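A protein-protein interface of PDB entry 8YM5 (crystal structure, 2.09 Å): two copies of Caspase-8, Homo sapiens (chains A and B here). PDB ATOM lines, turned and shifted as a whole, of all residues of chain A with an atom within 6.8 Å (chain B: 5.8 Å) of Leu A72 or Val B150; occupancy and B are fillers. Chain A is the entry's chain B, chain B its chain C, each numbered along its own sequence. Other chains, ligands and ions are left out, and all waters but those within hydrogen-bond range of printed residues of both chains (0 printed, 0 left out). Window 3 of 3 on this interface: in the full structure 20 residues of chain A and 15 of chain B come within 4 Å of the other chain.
Leu A72 touches just these residues of chain B: Lys B148 (3.0 Å), Arg B149 (3.3 Å) and Val B150 (3.5 Å). Of chain A, only Leu A72 and Asp A73 come within 4 Å of Val B150. Of the printed residues of chain B, Asn A70 touches Lys B148 (3.2 Å) and Arg B149 (3.8 Å). Printed residues of chain B within 4 Å of Arg A71: Lys B148 (3.5 Å). The nearest residue of chain A that does not touch Val B150 is Ile A76 (4.4 Å).
Printed residues of chain A that touch a printed residue of chain B: Asn A70, Arg A71, Leu A72 and Asp A73. Of the 9 printed residues of chain B, 4 touch a printed residue of chain A. Hydrophobic or aromatic side chains of chain B that line the printed part of chain A: Val B150. Among the printed residues, 9 pairs touch across the chains. Among the printed residues, no Asp or Glu carboxylate lies within 4 Å of a Lys or Arg side-chain nitrogen of the other chain.
O of Asp A73 sits at hydrogen-bond distance from OG1 of Thr A77 (2.7 Å). The side-chain carboxylate of Glu B145 is in salt-bridge range of the guanidinium group of Arg B149 (2.7 Å). NE of Arg A71 lies within salt-bridge range of OD1 of Asp A73, at 3.0 Å. N of Arg A71 lies within hydrogen-bond range of O of Leu A66, at 3.0 Å.
O of Lys B148 lies within hydrogen-bond range of N of Asp A73, at 3.0 Å. O of Lys B148 lies close to O of Asn A70. N of Leu A72 sits at hydrogen-bond distance from O of Lys B148, at 3.0 Å.
No position is printed for both chains. Of the 9 pairs that touch across the chains among the printed residues, none has its exchanged pair printed and touching as well.
Among the printed residues, pairs that only touch across the chains: Asp A73 with Val B150 (3.3 Å), Leu A72 with Arg B149 (3.3 Å), Arg A71 with Lys B148 (3.5 Å), Leu A72 with Val B150 (3.5 Å), Asp A73 with Glu B147 (3.6 Å) and Asn A70 with Arg B149 (3.8 Å).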
ATOM      1  N   LEU A  66      16.122  -3.237 -23.654  1.00  0.00           N
ATOM      2  CA  LEU A  66      17.076  -4.285 -23.315  1.00  0.00           C
ATOM      3  C   LEU A  66      17.762  -4.841 -24.564  1.00  0.00           C
ATOM      4  O   LEU A  66      18.952  -5.176 -24.521  1.00  0.00           O
ATOM      5  CB  LEU A  66      16.363  -5.391 -22.538  1.00  0.00           C
ATOM      6  CG  LEU A  66      15.859  -4.957 -21.146  1.00  0.00           C
ATOM      7  CD1 LEU A  66      15.109  -6.099 -20.471  1.00  0.00           C
ATOM      8  CD2 LEU A  66      17.032  -4.513 -20.286  1.00  0.00           C
ATOM      9  N   PHE A  67      17.042  -4.927 -25.688  1.00  0.00           N
ATOM     10  CA  PHE A  67      17.658  -5.380 -26.929  1.00  0.00           C
ATOM     11  C   PHE A  67      18.746  -4.411 -27.379  1.00  0.00           C
ATOM     12  O   PHE A  67      19.866  -4.825 -27.709  1.00  0.00           O
ATOM     13  CB  PHE A  67      16.589  -5.547 -28.021  1.00  0.00           C
ATOM     14  CG  PHE A  67      17.145  -6.040 -29.331  1.00  0.00           C
ATOM     15  CD1 PHE A  67      17.574  -7.356 -29.467  1.00  0.00           C
ATOM     16  CD2 PHE A  67      17.271  -5.183 -30.411  1.00  0.00           C
ATOM     17  CE1 PHE A  67      18.104  -7.827 -30.678  1.00  0.00           C
ATOM     18  CE2 PHE A  67      17.797  -5.646 -31.635  1.00  0.00           C
ATOM     19  CZ  PHE A  67      18.222  -6.972 -31.755  1.00  0.00           C
ATOM     20  N   ARG A  68      18.452  -3.107 -27.342  1.00  0.00           N
ATOM     21  CA  ARG A  68      19.390  -2.115 -27.853  1.00  0.00           C
ATOM     22  C   ARG A  68      20.628  -1.956 -26.967  1.00  0.00           C
ATOM     23  O   ARG A  68      21.666  -1.524 -27.471  1.00  0.00           O
ATOM     24  CB  ARG A  68      18.691  -0.770 -28.047  1.00  0.00           C
ATOM     25  CG  ARG A  68      17.688  -0.750 -29.212  1.00  0.00           C
ATOM     26  CD  ARG A  68      18.319  -1.241 -30.522  1.00  0.00           C
ATOM     27  NE  ARG A  68      17.382  -1.154 -31.636  1.00  0.00           N
ATOM     28  CZ  ARG A  68      17.617  -1.638 -32.849  1.00  0.00           C
ATOM     29  NH1 ARG A  68      18.744  -2.263 -33.140  1.00  0.00           N
ATOM     30  NH2 ARG A  68      16.699  -1.486 -33.795  1.00  0.00           N
ATOM     31  N   ILE A  69      20.562  -2.289 -25.678  1.00  0.00           N
ATOM     32  CA  ILE A  69      21.781  -2.292 -24.855  1.00  0.00           C
ATOM     33  C   ILE A  69      22.402  -3.683 -24.770  1.00  0.00           C
ATOM     34  O   ILE A  69      23.291  -3.911 -23.953  1.00  0.00           O
ATOM     35  CB  ILE A  69      21.550  -1.707 -23.441  1.00  0.00           C
ATOM     36  CG1 ILE A  69      20.577  -2.543 -22.599  1.00  0.00           C
ATOM     37  CG2 ILE A  69      21.030  -0.269 -23.513  1.00  0.00           C
ATOM     38  CD1 ILE A  69      20.706  -2.246 -21.062  1.00  0.00           C
ATOM     39  N   ASN A  70      21.962  -4.617 -25.620  1.00  0.00           N
ATOM     40  CA  ASN A  70      22.592  -5.926 -25.776  1.00  0.00           C
ATOM     41  C   ASN A  70      22.500  -6.776 -24.520  1.00  0.00           C
ATOM     42  O   ASN A  70      23.378  -7.596 -24.260  1.00  0.00           O
ATOM     43  CB  ASN A  70      24.058  -5.793 -26.220  1.00  0.00           C
ATOM     44  CG  ASN A  70      24.166  -5.237 -27.627  1.00  0.00           C
ATOM     45  OD1 ASN A  70      23.672  -5.848 -28.576  1.00  0.00           O
ATOM     46  ND2 ASN A  70      24.782  -4.073 -27.767  1.00  0.00           N
ATOM     47  N   ARG A  71      21.414  -6.631 -23.777  1.00  0.00           N
ATOM     48  CA  ARG A  71      21.121  -7.502 -22.639  1.00  0.00           C
ATOM     49  C   ARG A  71      20.185  -8.633 -23.069  1.00  0.00           C
ATOM     50  O   ARG A  71      19.030  -8.744 -22.639  1.00  0.00           O
ATOM     51  CB  ARG A  71      20.531  -6.687 -21.495  1.00  0.00           C
ATOM     52  CG  ARG A  71      21.534  -5.714 -20.803  1.00  0.00           C
ATOM     53  CD  ARG A  71      22.856  -6.396 -20.400  1.00  0.00           C
ATOM     54  NE  ARG A  71      22.647  -7.421 -19.379  1.00  0.00           N
ATOM     55  CZ  ARG A  71      22.734  -7.202 -18.071  1.00  0.00           C
ATOM     56  NH1 ARG A  71      23.011  -5.995 -17.590  1.00  0.00           N
ATOM     57  NH2 ARG A  71      22.542  -8.215 -17.229  1.00  0.00           N
ATOM     58  N   LEU A  72      20.690  -9.452 -23.989  1.00  0.00           N
ATOM     59  CA  LEU A  72      19.907 -10.585 -24.475  1.00  0.00           C
ATOM     60  C   LEU A  72      19.687 -11.617 -23.376  1.00  0.00           C
ATOM     61  O   LEU A  72      18.686 -12.351 -23.403  1.00  0.00           O
ATOM     62  CB  LEU A  72      20.604 -11.232 -25.675  1.00  0.00           C
ATOM     63  CG  LEU A  72      20.966 -10.340 -26.867  1.00  0.00           C
ATOM     64  CD1 LEU A  72      21.676 -11.123 -27.973  1.00  0.00           C
ATOM     65  CD2 LEU A  72      19.722  -9.701 -27.410  1.00  0.00           C
ATOM     66  N   ASP A  73      20.624 -11.703 -22.422  1.00  0.00           N
ATOM     67  CA  ASP A  73      20.469 -12.598 -21.274  1.00  0.00           C
ATOM     68  C   ASP A  73      19.193 -12.284 -20.514  1.00  0.00           C
ATOM     69  O   ASP A  73      18.437 -13.190 -20.129  1.00  0.00           O
ATOM     70  CB  ASP A  73      21.703 -12.498 -20.336  1.00  0.00           C
ATOM     71  CG  ASP A  73      21.904 -11.076 -19.709  1.00  0.00           C
ATOM     72  OD1 ASP A  73      21.581 -10.036 -20.357  1.00  0.00           O
ATOM     73  OD2 ASP A  73      22.420 -11.001 -18.555  1.00  0.00           O
ATOM     74  N   LEU A  74      18.933 -10.997 -20.287  1.00  0.00           N
ATOM     75  CA  LEU A  74      17.732 -10.592 -19.563  1.00  0.00           C
ATOM     76  C   LEU A  74      16.475 -10.818 -20.396  1.00  0.00           C
ATOM     77  O   LEU A  74      15.432 -11.229 -19.865  1.00  0.00           O
ATOM     78  CB  LEU A  74      17.854  -9.125 -19.144  1.00  0.00           C
ATOM     79  CG  LEU A  74      19.017  -8.790 -18.187  1.00  0.00           C
ATOM     80  CD1 LEU A  74      18.962  -7.328 -17.792  1.00  0.00           C
ATOM     81  CD2 LEU A  74      19.003  -9.682 -16.962  1.00  0.00           C
ATOM     82  N   LEU A  75      16.549 -10.527 -21.695  1.00  0.00           N
ATOM     83  CA  LEU A  75      15.424 -10.794 -22.595  1.00  0.00           C
ATOM     84  C   LEU A  75      14.996 -12.255 -22.516  1.00  0.00           C
ATOM     85  O   LEU A  75      13.807 -12.560 -22.346  1.00  0.00           O
ATOM     86  CB  LEU A  75      15.805 -10.426 -24.028  1.00  0.00           C
ATOM     87  CG  LEU A  75      15.716  -8.940 -24.341  1.00  0.00           C
ATOM     88  CD1 LEU A  75      16.337  -8.636 -25.711  1.00  0.00           C
ATOM     89  CD2 LEU A  75      14.246  -8.465 -24.277  1.00  0.00           C
ATOM     90  N   ILE A  76      15.959 -13.177 -22.602  1.00  0.00           N
ATOM     91  CA  ILE A  76      15.577 -14.587 -22.580  1.00  0.00           C
ATOM     92  C   ILE A  76      15.183 -15.040 -21.172  1.00  0.00           C
ATOM     93  O   ILE A  76      14.200 -15.767 -21.003  1.00  0.00           O
ATOM     94  CB  ILE A  76      16.688 -15.468 -23.174  1.00  0.00           C
ATOM     95  CG1 ILE A  76      16.306 -16.923 -22.986  1.00  0.00           C
ATOM     96  CG2 ILE A  76      18.005 -15.235 -22.458  1.00  0.00           C
ATOM     97  CD1 ILE A  76      15.300 -17.388 -24.000  1.00  0.00           C
ATOM     98  N   THR A  77      15.905 -14.593 -20.137  1.00  0.00           N
ATOM     99  CA  THR A  77      15.675 -15.121 -18.796  1.00  0.00           C
ATOM    100  C   THR A  77      14.373 -14.593 -18.202  1.00  0.00           C
ATOM    101  O   THR A  77      13.598 -15.357 -17.617  1.00  0.00           O
ATOM    102  CB  THR A  77      16.865 -14.757 -17.893  1.00  0.00           C
ATOM    103  OG1 THR A  77      18.049 -15.324 -18.449  1.00  0.00           O
ATOM    104  CG2 THR A  77      16.704 -15.304 -16.480  1.00  0.00           C
ATOM    105  N   THR A  81      12.153 -13.958 -24.528  1.00  0.00           N
ATOM    106  CA  THR A  81      12.279 -13.354 -25.846  1.00  0.00           C
ATOM    107  C   THR A  81      13.674 -13.615 -26.387  1.00  0.00           C
ATOM    108  O   THR A  81      14.670 -13.356 -25.703  1.00  0.00           O
ATOM    109  CB  THR A  81      11.982 -11.848 -25.780  1.00  0.00           C
ATOM    110  OG1 THR A  81      10.693 -11.664 -25.192  1.00  0.00           O
ATOM    111  CG2 THR A  81      11.971 -11.206 -27.169  1.00  0.00           C
ATOM    112  N   ARG A  82      13.698 -14.139 -27.615  1.00  0.00           N
ATOM    113  CA  ARG A  82      14.987 -14.464 -28.263  1.00  0.00           C
ATOM    114  C   ARG A  82      15.381 -13.335 -29.217  1.00  0.00           C
ATOM    115  O   ARG A  82      14.493 -12.553 -29.623  1.00  0.00           O
ATOM    116  CB  ARG A  82      14.878 -15.791 -29.022  1.00  0.00           C
ATOM    117  CG  ARG A  82      14.516 -16.969 -28.130  1.00  0.00           C
ATOM    118  CD  ARG A  82      14.444 -18.265 -28.917  1.00  0.00           C
ATOM    119  NE  ARG A  82      14.136 -19.415 -28.059  1.00  0.00           N
ATOM    120  CZ  ARG A  82      14.021 -20.664 -28.490  1.00  0.00           C
ATOM    121  NH1 ARG A  82      14.179 -20.937 -29.773  1.00  0.00           N
ATOM    122  NH2 ARG A  82      13.749 -21.635 -27.638  1.00  0.00           N
ATOM    123  N   LYS A  83      16.660 -13.271 -29.559  1.00  0.00           N
ATOM    124  CA  LYS A  83      17.204 -12.253 -30.455  1.00  0.00           C
ATOM    125  C   LYS A  83      16.440 -12.185 -31.781  1.00  0.00           C
ATOM    126  O   LYS A  83      16.096 -11.091 -32.252  1.00  0.00           O
ATOM    127  CB  LYS A  83      18.680 -12.565 -30.715  1.00  0.00           C
ATOM    128  CG  LYS A  83      19.439 -11.476 -31.422  1.00  0.00           C
ATOM    129  CD  LYS A  83      20.899 -11.877 -31.636  1.00  0.00           C
ATOM    130  CE  LYS A  83      21.617 -10.811 -32.446  1.00  0.00           C
ATOM    131  NZ  LYS A  83      22.885 -11.280 -33.044  1.00  0.00           N
ATOM    132  N   MET A  86      13.196 -10.332 -31.705  1.00  0.00           N
ATOM    133  CA  MET A  86      13.379  -8.881 -31.574  1.00  0.00           C
ATOM    134  C   MET A  86      13.767  -8.262 -32.903  1.00  0.00           C
ATOM    135  O   MET A  86      13.266  -7.192 -33.262  1.00  0.00           O
ATOM    136  CB  MET A  86      14.453  -8.536 -30.518  1.00  0.00           C
ATOM    137  CG  MET A  86      14.019  -8.592 -29.076  1.00  0.00           C
ATOM    138  SD  MET A  86      12.271  -7.840 -28.714  1.00  0.00           S
ATOM    139  CE  MET A  86      12.743  -5.965 -29.152  1.00  0.00           C
ATOM    140  N   GLU B 145      30.536 -10.101 -20.356  1.00  0.00           N
ATOM    141  CA  GLU B 145      29.961  -9.425 -21.515  1.00  0.00           C
ATOM    142  C   GLU B 145      29.430 -10.429 -22.546  1.00  0.00           C
ATOM    143  O   GLU B 145      28.372 -10.218 -23.144  1.00  0.00           O
ATOM    144  CB  GLU B 145      31.012  -8.496 -22.120  1.00  0.00           C
ATOM    145  CG  GLU B 145      30.545  -7.708 -23.347  1.00  0.00           C
ATOM    146  CD  GLU B 145      29.263  -6.933 -23.080  1.00  0.00           C
ATOM    147  OE1 GLU B 145      28.291  -7.103 -23.861  1.00  0.00           O
ATOM    148  OE2 GLU B 145      29.217  -6.221 -22.043  1.00  0.00           O
ATOM    149  N   MET B 146      30.142 -11.530 -22.755  1.00  0.00           N
ATOM    150  CA  MET B 146      29.716 -12.554 -23.704  1.00  0.00           C
ATOM    151  C   MET B 146      28.415 -13.188 -23.216  1.00  0.00           C
ATOM    152  O   MET B 146      27.531 -13.485 -24.005  1.00  0.00           O
ATOM    153  CB  MET B 146      30.799 -13.627 -23.891  1.00  0.00           C
ATOM    154  CG  MET B 146      32.036 -13.146 -24.652  1.00  0.00           C
ATOM    155  SD  MET B 146      33.496 -14.473 -24.611  1.00  0.00           S
ATOM    156  CE  MET B 146      32.749 -15.748 -25.958  1.00  0.00           C
ATOM    157  N   GLU B 147      28.312 -13.398 -21.902  1.00  0.00           N
ATOM    158  CA  GLU B 147      27.103 -13.993 -21.344  1.00  0.00           C
ATOM    159  C   GLU B 147      25.907 -13.067 -21.517  1.00  0.00           C
ATOM    160  O   GLU B 147      24.784 -13.532 -21.768  1.00  0.00           O
ATOM    161  CB  GLU B 147      27.311 -14.330 -19.857  1.00  0.00           C
ATOM    162  CG  GLU B 147      28.126 -15.618 -19.627  1.00  0.00           C
ATOM    163  CD  GLU B 147      28.229 -16.011 -18.149  1.00  0.00           C
ATOM    164  OE1 GLU B 147      27.899 -15.191 -17.277  1.00  0.00           O
ATOM    165  OE2 GLU B 147      28.670 -17.138 -17.851  1.00  0.00           O
ATOM    166  N   LYS B 148      26.121 -11.759 -21.347  1.00  0.00           N
ATOM    167  CA  LYS B 148      25.043 -10.800 -21.554  1.00  0.00           C
ATOM    168  C   LYS B 148      24.536 -10.836 -22.976  1.00  0.00           C
ATOM    169  O   LYS B 148      23.340 -10.602 -23.225  1.00  0.00           O
ATOM    170  CB  LYS B 148      25.519  -9.385 -21.231  1.00  0.00           C
ATOM    171  CG  LYS B 148      25.697  -9.127 -19.769  1.00  0.00           C
ATOM    172  CD  LYS B 148      26.349  -7.758 -19.570  1.00  0.00           C
ATOM    173  CE  LYS B 148      26.513  -7.468 -18.071  1.00  0.00           C
ATOM    174  NZ  LYS B 148      27.330  -6.233 -17.842  1.00  0.00           N
ATOM    175  N   ARG B 149      25.430 -11.079 -23.927  1.00  0.00           N
ATOM    176  CA  ARG B 149      25.020 -11.173 -25.313  1.00  0.00           C
ATOM    177  C   ARG B 149      24.628 -12.588 -25.684  1.00  0.00           C
ATOM    178  O   ARG B 149      24.326 -12.835 -26.849  1.00  0.00           O
ATOM    179  CB  ARG B 149      26.138 -10.692 -26.232  1.00  0.00           C
ATOM    180  CG  ARG B 149      26.395  -9.224 -26.157  1.00  0.00           C
ATOM    181  CD  ARG B 149      27.729  -8.927 -26.809  1.00  0.00           C
ATOM    182  NE  ARG B 149      28.170  -7.569 -26.522  1.00  0.00           N
ATOM    183  CZ  ARG B 149      28.061  -6.562 -27.375  1.00  0.00           C
ATOM    184  NH1 ARG B 149      27.548  -6.733 -28.582  1.00  0.00           N
ATOM    185  NH2 ARG B 149      28.482  -5.354 -27.006  1.00  0.00           N
ATOM    186  N   VAL B 150      24.606 -13.502 -24.709  1.00  0.00           N
ATOM    187  CA  VAL B 150      24.260 -14.907 -24.899  1.00  0.00           C
ATOM    188  C   VAL B 150      25.066 -15.507 -26.052  1.00  0.00           C
ATOM    189  O   VAL B 150      24.553 -16.309 -26.832  1.00  0.00           O
ATOM    190  CB  VAL B 150      22.734 -15.069 -25.118  1.00  0.00           C
ATOM    191  CG1 VAL B 150      22.286 -16.505 -24.913  1.00  0.00           C
ATOM    192  CG2 VAL B 150      21.974 -14.211 -24.117  1.00  0.00           C
ATOM    193  N   ILE B 151      26.342 -15.141 -26.168  1.00  0.00           N
ATOM    194  CA  ILE B 151      27.239 -15.879 -27.050  1.00  0.00           C
ATOM    195  C   ILE B 151      28.166 -16.777 -26.253  1.00  0.00           C
ATOM    196  O   ILE B 151      29.089 -17.375 -26.815  1.00  0.00           O
ATOM    197  CB  ILE B 151      28.020 -14.942 -27.979  1.00  0.00           C
ATOM    198  CG1 ILE B 151      28.929 -14.017 -27.163  1.00  0.00           C
ATOM    199  CG2 ILE B 151      27.045 -14.178 -28.920  1.00  0.00           C
ATOM    200  CD1 ILE B 151      29.829 -13.140 -28.015  1.00  0.00           C
ATOM    201  N   LEU B 152      27.919 -16.900 -24.949  1.00  0.00           N
ATOM    202  CA  LEU B 152      28.657 -17.775 -24.052  1.00  0.00           C
ATOM    203  C   LEU B 152      27.669 -18.282 -23.020  1.00  0.00           C
ATOM    204  O   LEU B 152      26.939 -17.480 -22.434  1.00  0.00           O
ATOM    205  CB  LEU B 152      29.808 -17.020 -23.347  1.00  0.00           C
ATOM    206  CG  LEU B 152      30.594 -17.841 -22.323  1.00  0.00           C
ATOM    207  CD1 LEU B 152      31.250 -19.025 -23.026  1.00  0.00           C
ATOM    208  CD2 LEU B 152      31.655 -16.975 -21.562  1.00  0.00           C
ATOM    209  N   LYS B 156      26.491 -23.058 -24.956  1.00  0.00           N
ATOM    210  CA  LYS B 156      26.959 -22.182 -26.036  1.00  0.00           C
ATOM    211  C   LYS B 156      28.458 -21.977 -25.862  1.00  0.00           C
ATOM    212  O   LYS B 156      28.912 -20.943 -25.368  1.00  0.00           O
ATOM    213  CB  LYS B 156      26.184 -20.847 -25.990  1.00  0.00           C
ATOM    214  CG  LYS B 156      24.724 -20.998 -26.390  1.00  0.00           C
ATOM    215  CD  LYS B 156      23.940 -19.699 -26.296  1.00  0.00           C
ATOM    216  CE  LYS B 156      22.510 -19.963 -25.824  1.00  0.00           C
ATOM    217  NZ  LYS B 156      22.410 -19.843 -24.338  1.00  0.00           N
